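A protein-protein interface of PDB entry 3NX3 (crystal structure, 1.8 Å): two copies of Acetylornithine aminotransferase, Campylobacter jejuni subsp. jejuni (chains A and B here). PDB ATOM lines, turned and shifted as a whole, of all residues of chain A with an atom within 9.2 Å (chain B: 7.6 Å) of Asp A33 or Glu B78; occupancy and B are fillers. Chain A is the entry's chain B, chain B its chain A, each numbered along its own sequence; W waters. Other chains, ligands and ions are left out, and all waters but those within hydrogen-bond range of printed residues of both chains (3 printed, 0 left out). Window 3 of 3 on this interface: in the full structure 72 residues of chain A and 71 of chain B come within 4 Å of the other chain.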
ATOM      1  N   ASP A  19      -2.768   7.388  14.402  1.00  0.00           N
ATOM      2  CA  ASP A  19      -3.642   8.289  13.654  1.00  0.00           C
ATOM      3  C   ASP A  19      -4.698   8.889  14.573  1.00  0.00           C
ATOM      4  O   ASP A  19      -5.902   8.758  14.339  1.00  0.00           O
ATOM      5  CB  ASP A  19      -4.309   7.564  12.475  1.00  0.00           C
ATOM      6  CG  ASP A  19      -5.240   6.443  12.919  1.00  0.00           C
ATOM      7  OD1 ASP A  19      -4.916   5.737  13.900  1.00  0.00           O
ATOM      8  OD2 ASP A  19      -6.304   6.270  12.283  1.00  0.00           O
ATOM      9  N   ILE A  20      -4.233   9.547  15.627  1.00  0.00           N
ATOM     10  CA  ILE A  20      -5.117  10.154  16.606  1.00  0.00           C
ATOM     11  C   ILE A  20      -4.579  11.540  16.902  1.00  0.00           C
ATOM     12  O   ILE A  20      -3.402  11.694  17.216  1.00  0.00           O
ATOM     13  CB  ILE A  20      -5.152   9.341  17.915  1.00  0.00           C
ATOM     14  CG1 ILE A  20      -5.695   7.933  17.660  1.00  0.00           C
ATOM     15  CG2 ILE A  20      -5.997  10.042  18.964  1.00  0.00           C
ATOM     16  CD1 ILE A  20      -5.706   7.059  18.896  1.00  0.00           C
ATOM     17  N   VAL A  21      -5.444  12.542  16.764  1.00  0.00           N
ATOM     18  CA  VAL A  21      -5.121  13.919  17.114  1.00  0.00           C
ATOM     19  C   VAL A  21      -5.688  14.203  18.505  1.00  0.00           C
ATOM     20  O   VAL A  21      -6.907  14.223  18.692  1.00  0.00           O
ATOM     21  CB  VAL A  21      -5.780  14.891  16.114  1.00  0.00           C
ATOM     22  CG1 VAL A  21      -5.387  16.331  16.409  1.00  0.00           C
ATOM     23  CG2 VAL A  21      -5.430  14.495  14.679  1.00  0.00           C
ATOM     24  N   LEU A  22      -4.812  14.396  19.485  1.00  0.00           N
ATOM     25  CA  LEU A  22      -5.276  14.672  20.837  1.00  0.00           C
ATOM     26  C   LEU A  22      -5.509  16.167  21.007  1.00  0.00           C
ATOM     27  O   LEU A  22      -4.707  16.986  20.565  1.00  0.00           O
ATOM     28  CB  LEU A  22      -4.300  14.154  21.881  1.00  0.00           C
ATOM     29  CG  LEU A  22      -4.157  12.635  21.953  1.00  0.00           C
ATOM     30  CD1 LEU A  22      -3.136  12.272  23.043  1.00  0.00           C
ATOM     31  CD2 LEU A  22      -5.521  11.980  22.213  1.00  0.00           C
ATOM     32  N   GLU A  23      -6.621  16.516  21.645  1.00  0.00           N
ATOM     33  CA  GLU A  23      -6.997  17.920  21.790  1.00  0.00           C
ATOM     34  C   GLU A  23      -6.983  18.397  23.239  1.00  0.00           C
ATOM     35  O   GLU A  23      -6.501  19.487  23.534  1.00  0.00           O
ATOM     36  CB  GLU A  23      -8.367  18.175  21.152  1.00  0.00           C
ATOM     37  CG  GLU A  23      -8.906  19.560  21.431  1.00  0.00           C
ATOM     38  CD  GLU A  23      -9.900  20.022  20.391  1.00  0.00           C
ATOM     39  OE1 GLU A  23     -10.148  19.262  19.428  1.00  0.00           O
ATOM     40  OE2 GLU A  23     -10.428  21.150  20.537  1.00  0.00           O
ATOM     41  N   LYS A  24      -7.509  17.581  24.145  1.00  0.00           N
ATOM     42  CA  LYS A  24      -7.589  17.965  25.549  1.00  0.00           C
ATOM     43  C   LYS A  24      -7.734  16.740  26.429  1.00  0.00           C
ATOM     44  O   LYS A  24      -7.849  15.631  25.938  1.00  0.00           O
ATOM     45  CB  LYS A  24      -8.768  18.914  25.785  1.00  0.00           C
ATOM     46  CG  LYS A  24     -10.121  18.273  25.542  1.00  0.00           C
ATOM     47  CD  LYS A  24     -11.250  19.285  25.681  1.00  0.00           C
ATOM     48  CE  LYS A  24     -11.154  20.360  24.606  1.00  0.00           C
ATOM     49  NZ  LYS A  24     -12.365  21.231  24.570  1.00  0.00           N
ATOM     50  N   LEU A  30      -8.311  11.295  28.012  1.00  0.00           N
ATOM     51  CA  LEU A  30      -7.885  12.163  26.911  1.00  0.00           C
ATOM     52  C   LEU A  30      -8.965  12.190  25.844  1.00  0.00           C
ATOM     53  O   LEU A  30      -9.699  11.217  25.671  1.00  0.00           O
ATOM     54  CB  LEU A  30      -6.564  11.679  26.302  1.00  0.00           C
ATOM     55  CG  LEU A  30      -5.310  12.052  27.100  1.00  0.00           C
ATOM     56  CD1 LEU A  30      -4.126  11.169  26.721  1.00  0.00           C
ATOM     57  CD2 LEU A  30      -4.995  13.544  26.923  1.00  0.00           C
ATOM     58  N   PHE A  31      -9.065  13.307  25.128  1.00  0.00           N
ATOM     59  CA  PHE A  31     -10.073  13.450  24.086  1.00  0.00           C
ATOM     60  C   PHE A  31      -9.433  13.794  22.751  1.00  0.00           C
ATOM     61  O   PHE A  31      -8.562  14.671  22.678  1.00  0.00           O
ATOM     62  CB  PHE A  31     -11.064  14.557  24.461  1.00  0.00           C
ATOM     63  CG  PHE A  31     -11.821  14.286  25.725  1.00  0.00           C
ATOM     64  CD1 PHE A  31     -13.097  13.753  25.683  1.00  0.00           C
ATOM     65  CD2 PHE A  31     -11.252  14.559  26.961  1.00  0.00           C
ATOM     66  CE1 PHE A  31     -13.796  13.505  26.851  1.00  0.00           C
ATOM     67  CE2 PHE A  31     -11.947  14.310  28.129  1.00  0.00           C
ATOM     68  CZ  PHE A  31     -13.218  13.778  28.073  1.00  0.00           C
ATOM     69  N   ASP A  32      -9.873  13.130  21.688  1.00  0.00           N
ATOM     70  CA  ASP A  32      -9.333  13.439  20.370  1.00  0.00           C
ATOM     71  C   ASP A  32     -10.120  14.568  19.686  1.00  0.00           C
ATOM     72  O   ASP A  32     -11.029  15.151  20.283  1.00  0.00           O
ATOM     73  CB  ASP A  32      -9.211  12.189  19.485  1.00  0.00           C
ATOM     74  CG  ASP A  32     -10.560  11.652  19.008  1.00  0.00           C
ATOM     75  OD1 ASP A  32     -11.573  12.379  19.071  1.00  0.00           O
ATOM     76  OD2 ASP A  32     -10.591  10.487  18.550  1.00  0.00           O
ATOM     77  N   ASP A  33      -9.766  14.873  18.443  1.00  0.00           N
ATOM     78  CA  ASP A  33     -10.339  16.030  17.761  1.00  0.00           C
ATOM     79  C   ASP A  33     -11.778  15.777  17.306  1.00  0.00           C
ATOM     80  O   ASP A  33     -12.418  16.653  16.729  1.00  0.00           O
ATOM     81  CB  ASP A  33      -9.438  16.498  16.607  1.00  0.00           C
ATOM     82  CG  ASP A  33      -9.372  15.502  15.459  1.00  0.00           C
ATOM     83  OD1 ASP A  33      -9.766  14.332  15.646  1.00  0.00           O
ATOM     84  OD2 ASP A  33      -8.912  15.892  14.361  1.00  0.00           O
ATOM     85  N   LYS A  34     -12.282  14.578  17.583  1.00  0.00           N
ATOM     86  CA  LYS A  34     -13.674  14.246  17.315  1.00  0.00           C
ATOM     87  C   LYS A  34     -14.430  14.056  18.626  1.00  0.00           C
ATOM     88  O   LYS A  34     -15.540  13.517  18.644  1.00  0.00           O
ATOM     89  CB  LYS A  34     -13.775  12.981  16.462  1.00  0.00           C
ATOM     90  CG  LYS A  34     -13.154  13.111  15.085  1.00  0.00           C
ATOM     91  CD  LYS A  34     -13.345  11.835  14.282  1.00  0.00           C
ATOM     92  CE  LYS A  34     -12.812  11.983  12.864  1.00  0.00           C
ATOM     93  NZ  LYS A  34     -13.073  10.769  12.040  1.00  0.00           N
ATOM     94  N   ALA A  35     -13.806  14.496  19.715  1.00  0.00           N
ATOM     95  CA  ALA A  35     -14.390  14.425  21.052  1.00  0.00           C
ATOM     96  C   ALA A  35     -14.568  12.992  21.558  1.00  0.00           C
ATOM     97  O   ALA A  35     -15.356  12.743  22.471  1.00  0.00           O
ATOM     98  CB  ALA A  35     -15.714  15.191  21.107  1.00  0.00           C
ATOM     99  N   LYS A  36     -13.839  12.047  20.976  1.00  0.00           N
ATOM    100  CA  LYS A  36     -13.879  10.687  21.497  1.00  0.00           C
ATOM    101  C   LYS A  36     -13.066  10.637  22.783  1.00  0.00           C
ATOM    102  O   LYS A  36     -11.980  11.218  22.864  1.00  0.00           O
ATOM    103  CB  LYS A  36     -13.354   9.678  20.474  1.00  0.00           C
ATOM    104  CG  LYS A  36     -13.332   8.256  20.997  1.00  0.00           C
ATOM    105  CD  LYS A  36     -12.952   7.250  19.918  1.00  0.00           C
ATOM    106  CE  LYS A  36     -12.885   5.836  20.494  1.00  0.00           C
ATOM    107  NZ  LYS A  36     -12.546   4.813  19.470  1.00  0.00           N
ATOM    108  N   LYS A  37     -13.602   9.963  23.791  1.00  0.00           N
ATOM    109  CA  LYS A  37     -12.963   9.896  25.105  1.00  0.00           C
ATOM    110  C   LYS A  37     -12.172   8.596  25.281  1.00  0.00           C
ATOM    111  O   LYS A  37     -12.707   7.509  25.100  1.00  0.00           O
ATOM    112  CB  LYS A  37     -14.038  10.007  26.192  1.00  0.00           C
ATOM    113  CG  LYS A  37     -13.512  10.065  27.618  1.00  0.00           C
ATOM    114  CD  LYS A  37     -14.667  10.058  28.610  1.00  0.00           C
ATOM    115  CE  LYS A  37     -14.173  10.056  30.041  1.00  0.00           C
ATOM    116  NZ  LYS A  37     -15.281   9.990  31.030  1.00  0.00           N
ATOM    117  N   TYR A  38     -10.896   8.705  25.632  1.00  0.00           N
ATOM    118  CA  TYR A  38     -10.078   7.514  25.845  1.00  0.00           C
ATOM    119  C   TYR A  38      -9.575   7.479  27.273  1.00  0.00           C
ATOM    120  O   TYR A  38      -9.178   8.508  27.827  1.00  0.00           O
ATOM    121  CB  TYR A  38      -8.842   7.518  24.943  1.00  0.00           C
ATOM    122  CG  TYR A  38      -9.078   7.649  23.457  1.00  0.00           C
ATOM    123  CD1 TYR A  38      -8.893   6.563  22.613  1.00  0.00           C
ATOM    124  CD2 TYR A  38      -9.433   8.868  22.892  1.00  0.00           C
ATOM    125  CE1 TYR A  38      -9.073   6.679  21.248  1.00  0.00           C
ATOM    126  CE2 TYR A  38      -9.614   8.995  21.529  1.00  0.00           C
ATOM    127  CZ  TYR A  38      -9.439   7.899  20.714  1.00  0.00           C
ATOM    128  OH  TYR A  38      -9.628   8.013  19.351  1.00  0.00           O
ATOM    129  N   LYS B  67      -5.721  23.378  28.445  1.00  0.00           N
ATOM    130  CA  LYS B  67      -6.164  22.506  27.369  1.00  0.00           C
ATOM    131  C   LYS B  67      -5.359  21.203  27.380  1.00  0.00           C
ATOM    132  O   LYS B  67      -5.898  20.144  27.670  1.00  0.00           O
ATOM    133  CB  LYS B  67      -6.028  23.240  26.028  1.00  0.00           C
ATOM    134  CG  LYS B  67      -6.929  22.729  24.916  1.00  0.00           C
ATOM    135  CD  LYS B  67      -6.947  23.715  23.757  1.00  0.00           C
ATOM    136  CE  LYS B  67      -7.874  23.255  22.641  1.00  0.00           C
ATOM    137  NZ  LYS B  67      -7.254  22.179  21.819  1.00  0.00           N
ATOM    138  N   TYR B  76      -0.763  13.117  17.232  1.00  0.00           N
ATOM    139  CA  TYR B  76      -0.795  14.427  16.587  1.00  0.00           C
ATOM    140  C   TYR B  76      -1.431  15.465  17.498  1.00  0.00           C
ATOM    141  O   TYR B  76      -2.301  15.149  18.323  1.00  0.00           O
ATOM    142  CB  TYR B  76      -1.619  14.375  15.300  1.00  0.00           C
ATOM    143  CG  TYR B  76      -0.966  13.639  14.151  1.00  0.00           C
ATOM    144  CD1 TYR B  76      -0.010  14.258  13.355  1.00  0.00           C
ATOM    145  CD2 TYR B  76      -1.325  12.329  13.841  1.00  0.00           C
ATOM    146  CE1 TYR B  76       0.578  13.589  12.293  1.00  0.00           C
ATOM    147  CE2 TYR B  76      -0.740  11.659  12.791  1.00  0.00           C
ATOM    148  CZ  TYR B  76       0.209  12.290  12.018  1.00  0.00           C
ATOM    149  OH  TYR B  76       0.788  11.612  10.967  1.00  0.00           O
ATOM    150  N   ASN B  77      -1.006  16.713  17.327  1.00  0.00           N
ATOM    151  CA  ASN B  77      -1.661  17.831  17.982  1.00  0.00           C
ATOM    152  C   ASN B  77      -1.630  19.020  17.020  1.00  0.00           C
ATOM    153  O   ASN B  77      -0.596  19.295  16.405  1.00  0.00           O
ATOM    154  CB  ASN B  77      -0.969  18.145  19.312  1.00  0.00           C
ATOM    155  CG  ASN B  77      -1.657  19.242  20.083  1.00  0.00           C
ATOM    156  OD1 ASN B  77      -2.614  19.010  20.841  1.00  0.00           O
ATOM    157  ND2 ASN B  77      -1.167  20.447  19.912  1.00  0.00           N
ATOM    158  N   GLU B  78      -2.764  19.703  16.875  1.00  0.00           N
ATOM    159  CA  GLU B  78      -2.886  20.798  15.910  1.00  0.00           C
ATOM    160  C   GLU B  78      -1.896  21.936  16.176  1.00  0.00           C
ATOM    161  O   GLU B  78      -1.392  22.561  15.227  1.00  0.00           O
ATOM    162  CB  GLU B  78      -4.326  21.331  15.866  1.00  0.00           C
ATOM    163  CG  GLU B  78      -5.319  20.357  15.227  1.00  0.00           C
ATOM    164  CD  GLU B  78      -6.779  20.723  15.478  1.00  0.00           C
ATOM    165  OE1 GLU B  78      -7.108  21.929  15.533  1.00  0.00           O
ATOM    166  OE2 GLU B  78      -7.598  19.790  15.626  1.00  0.00           O
ATOM    167  N   ASN B  79      -1.620  22.211  17.454  1.00  0.00           N
ATOM    168  CA  ASN B  79      -0.669  23.288  17.782  1.00  0.00           C
ATOM    169  C   ASN B  79       0.698  23.018  17.172  1.00  0.00           C
ATOM    170  O   ASN B  79       1.379  23.928  16.706  1.00  0.00           O
ATOM    171  CB  ASN B  79      -0.471  23.461  19.294  1.00  0.00           C
ATOM    172  CG  ASN B  79      -1.704  24.002  19.998  1.00  0.00           C
ATOM    173  OD1 ASN B  79      -2.246  25.040  19.630  1.00  0.00           O
ATOM    174  ND2 ASN B  79      -2.151  23.290  21.016  1.00  0.00           N
ATOM    175  N   ILE B  80       1.118  21.763  17.230  1.00  0.00           N
ATOM    176  CA  ILE B  80       2.432  21.398  16.739  1.00  0.00           C
ATOM    177  C   ILE B  80       2.507  21.548  15.221  1.00  0.00           C
ATOM    178  O   ILE B  80       3.459  22.128  14.690  1.00  0.00           O
ATOM    179  CB  ILE B  80       2.794  19.981  17.212  1.00  0.00           C
ATOM    180  CG1 ILE B  80       2.749  19.940  18.745  1.00  0.00           C
ATOM    181  CG2 ILE B  80       4.143  19.574  16.677  1.00  0.00           C
ATOM    182  CD1 ILE B  80       2.894  18.522  19.345  1.00  0.00           C
ATOM    183  N   ALA B  81       1.487  21.065  14.520  1.00  0.00           N
ATOM    184  CA  ALA B  81       1.410  21.246  13.072  1.00  0.00           C
ATOM    185  C   ALA B  81       1.443  22.723  12.669  1.00  0.00           C
ATOM    186  O   ALA B  81       2.138  23.108  11.725  1.00  0.00           O
ATOM    187  CB  ALA B  81       0.167  20.580  12.510  1.00  0.00           C
ATOM    188  N   ALA B  82       0.689  23.552  13.381  1.00  0.00           N
ATOM    189  CA  ALA B  82       0.646  24.980  13.054  1.00  0.00           C
ATOM    190  C   ALA B  82       1.995  25.677  13.315  1.00  0.00           C
ATOM    191  O   ALA B  82       2.435  26.529  12.530  1.00  0.00           O
ATOM    192  CB  ALA B  82      -0.503  25.677  13.800  1.00  0.00           C
ATOM    193  N   ALA B  83       2.666  25.284  14.391  1.00  0.00           N
ATOM    194  CA  ALA B  83       3.968  25.854  14.722  1.00  0.00           C
ATOM    195  C   ALA B  83       5.023  25.460  13.692  1.00  0.00           C
ATOM    196  O   ALA B  83       5.829  26.284  13.276  1.00  0.00           O
ATOM    197  CB  ALA B  83       4.394  25.436  16.138  1.00  0.00           C
ATOM    198  N   ALA B  84       5.009  24.202  13.266  1.00  0.00           N
ATOM    199  CA  ALA B  84       5.923  23.760  12.216  1.00  0.00           C
ATOM    200  C   ALA B  84       5.688  24.525  10.907  1.00  0.00           C
ATOM    201  O   ALA B  84       6.632  24.935  10.234  1.00  0.00           O
ATOM    202  CB  ALA B  84       5.785  22.263  11.998  1.00  0.00           C
ATOM    203  N   PRO B 283       2.283  20.390  22.933  1.00  0.00           N
ATOM    204  CA  PRO B 283       1.244  21.391  22.659  1.00  0.00           C
ATOM    205  C   PRO B 283       1.471  22.725  23.345  1.00  0.00           C
ATOM    206  O   PRO B 283       1.145  23.742  22.747  1.00  0.00           O
ATOM    207  CB  PRO B 283      -0.025  20.735  23.195  1.00  0.00           C
ATOM    208  CG  PRO B 283       0.260  19.258  23.135  1.00  0.00           C
ATOM    209  CD  PRO B 283       1.717  19.107  23.399  1.00  0.00           C
ATOM    210  N   CYS B 286       4.572  24.624  21.577  1.00  0.00           N
ATOM    211  CA  CYS B 286       4.164  24.956  20.211  1.00  0.00           C
ATOM    212  C   CYS B 286       3.055  26.016  20.161  1.00  0.00           C
ATOM    213  O   CYS B 286       3.044  26.845  19.250  1.00  0.00           O
ATOM    214  CB  CYS B 286       3.791  23.706  19.434  1.00  0.00           C
ATOM    215  SG  CYS B 286       5.282  22.718  19.132  1.00  0.00           S
ATOM    216  N   ALA B 287       2.141  26.003  21.137  1.00  0.00           N
ATOM    217  CA  ALA B 287       1.212  27.129  21.294  1.00  0.00           C
ATOM    218  C   ALA B 287       2.003  28.423  21.511  1.00  0.00           C
ATOM    219  O   ALA B 287       1.644  29.487  21.005  1.00  0.00           O
ATOM    220  CB  ALA B 287       0.227  26.874  22.454  1.00  0.00           C
ATOM    221  N   ASN B 290       3.518  29.507  18.107  1.00  0.00           N
ATOM    222  CA  ASN B 290       2.490  30.140  17.284  1.00  0.00           C
ATOM    223  C   ASN B 290       2.203  31.543  17.761  1.00  0.00           C
ATOM    224  O   ASN B 290       2.058  32.450  16.944  1.00  0.00           O
ATOM    225  CB  ASN B 290       1.221  29.306  17.255  1.00  0.00           C
ATOM    226  CG  ASN B 290       1.413  28.040  16.464  1.00  0.00           C
ATOM    227  OD1 ASN B 290       2.122  28.043  15.465  1.00  0.00           O
ATOM    228  ND2 ASN B 290       0.819  26.949  16.921  1.00  0.00           N
HETATM  229  O   HOH W   1      -5.004  19.185  18.509  1.00  0.00           O
HETATM  230  O   HOH W   2      -7.671  19.341  18.013  1.00  0.00           O
HETATM  231  O   HOH W   3      -4.276  21.033  22.326  1.00  0.00           O
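Among the printed residues, pairs that only touch across the chains: Val A21 with Tyr B76 (3.3 Å), Lys A24 with Lys B67 (3.5 Å) and Asp A33 with Glu B78 (3.9 Å).
Along chain A the printed residues that touch a printed residue of chain B span positions 20 to 33. Printed residues of chain B that touch a printed residue of chain A: Lys B67, Tyr B76, Asn B77 and Glu B78. Hydrophobic or aromatic side chains of chain B within 4 Å of the printed part of chain A: Tyr B76. Among the printed residues, 7 pairs touch across the chains. Among the printed residues, Asp or Glu carboxylates within 4 Å of a Lys or Arg side-chain nitrogen of the other chain: Glu A23 with Lys B67.
The side-chain amino group (NZ) of Lys B67 is in salt-bridge range of the side-chain carboxylate (OE2) of Glu A23 (3.6 Å). The backbone NH (N) of Tyr B76 is in hydrogen-bond range of the backbone carbonyl oxygen (O) of Ile A20, at 3.0 Å. O of Tyr B76 lies within hydrogen-bond range of N of Leu A22 (2.9 Å). The side-chain amide oxygen of Asn B77 sits close to the backbone carbonyl oxygen of Leu A22, 2.9 Å away.
No position is printed for both chains. Of the 7 pairs that touch across the chains among the printed residues, none has its exchanged pair printed and touching as well.
The side-chain amide nitrogen (ND2) of Asn B77 sits close to the backbone NH (N) of Asn B79. The backbone carbonyl oxygen (O) of Val A21 is in hydrogen-bond range of the backbone NH (N) of Asp A33, 2.9 Å away. N of Glu A23 is in hydrogen-bond range of O of Phe A31, 2.9 Å away. The backbone NH (N) of Phe A31 sits at hydrogen-bond distance from the backbone carbonyl oxygen (O) of Lys A24 (2.7 Å).
Printed residues of chain B within 4 Å of Ile A20: Tyr B76. Printed residues of chain B within 4 Å of Val A21: Tyr B76. Of the printed residues of chain B, Asp A33 touches Glu B78 (3.9 Å). Ala A35 touches none of the printed residues of chain B. Printed residues of chain A within 4 Å of Glu B78: Asp A33 (3.9 Å). No residue of chain A comes within 4 Å of Asn B79. No residue of chain A comes within 4 Å of Ala B81. The nearest printed residue of chain A that does not touch Glu B78 is Val A21 (4.2 Å). The nearest printed residue of chain A that does not touch Lys B67 is Leu A22 (5.9 Å).
Water W2 bridges OE2 of Glu B78 (2.4 Å) and OE1 of Glu A23 (2.9 Å). Water W1 lies within hydrogen-bond range of the backbone NH of Glu B78 (2.8 Å), the backbone carbonyl oxygen of Leu A22 (3.0 Å) and the side-chain amide oxygen of Asn B77 (3.3 Å). Water W3 lies within hydrogen-bond range of the backbone carbonyl oxygen of Glu A23 (3.0 Å), the side-chain amide oxygen of Asn B77 (3.0 Å), the side-chain amino group of Lys B67 (3.2 Å) and the side-chain amide nitrogen of Asn B79 (3.4 Å).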
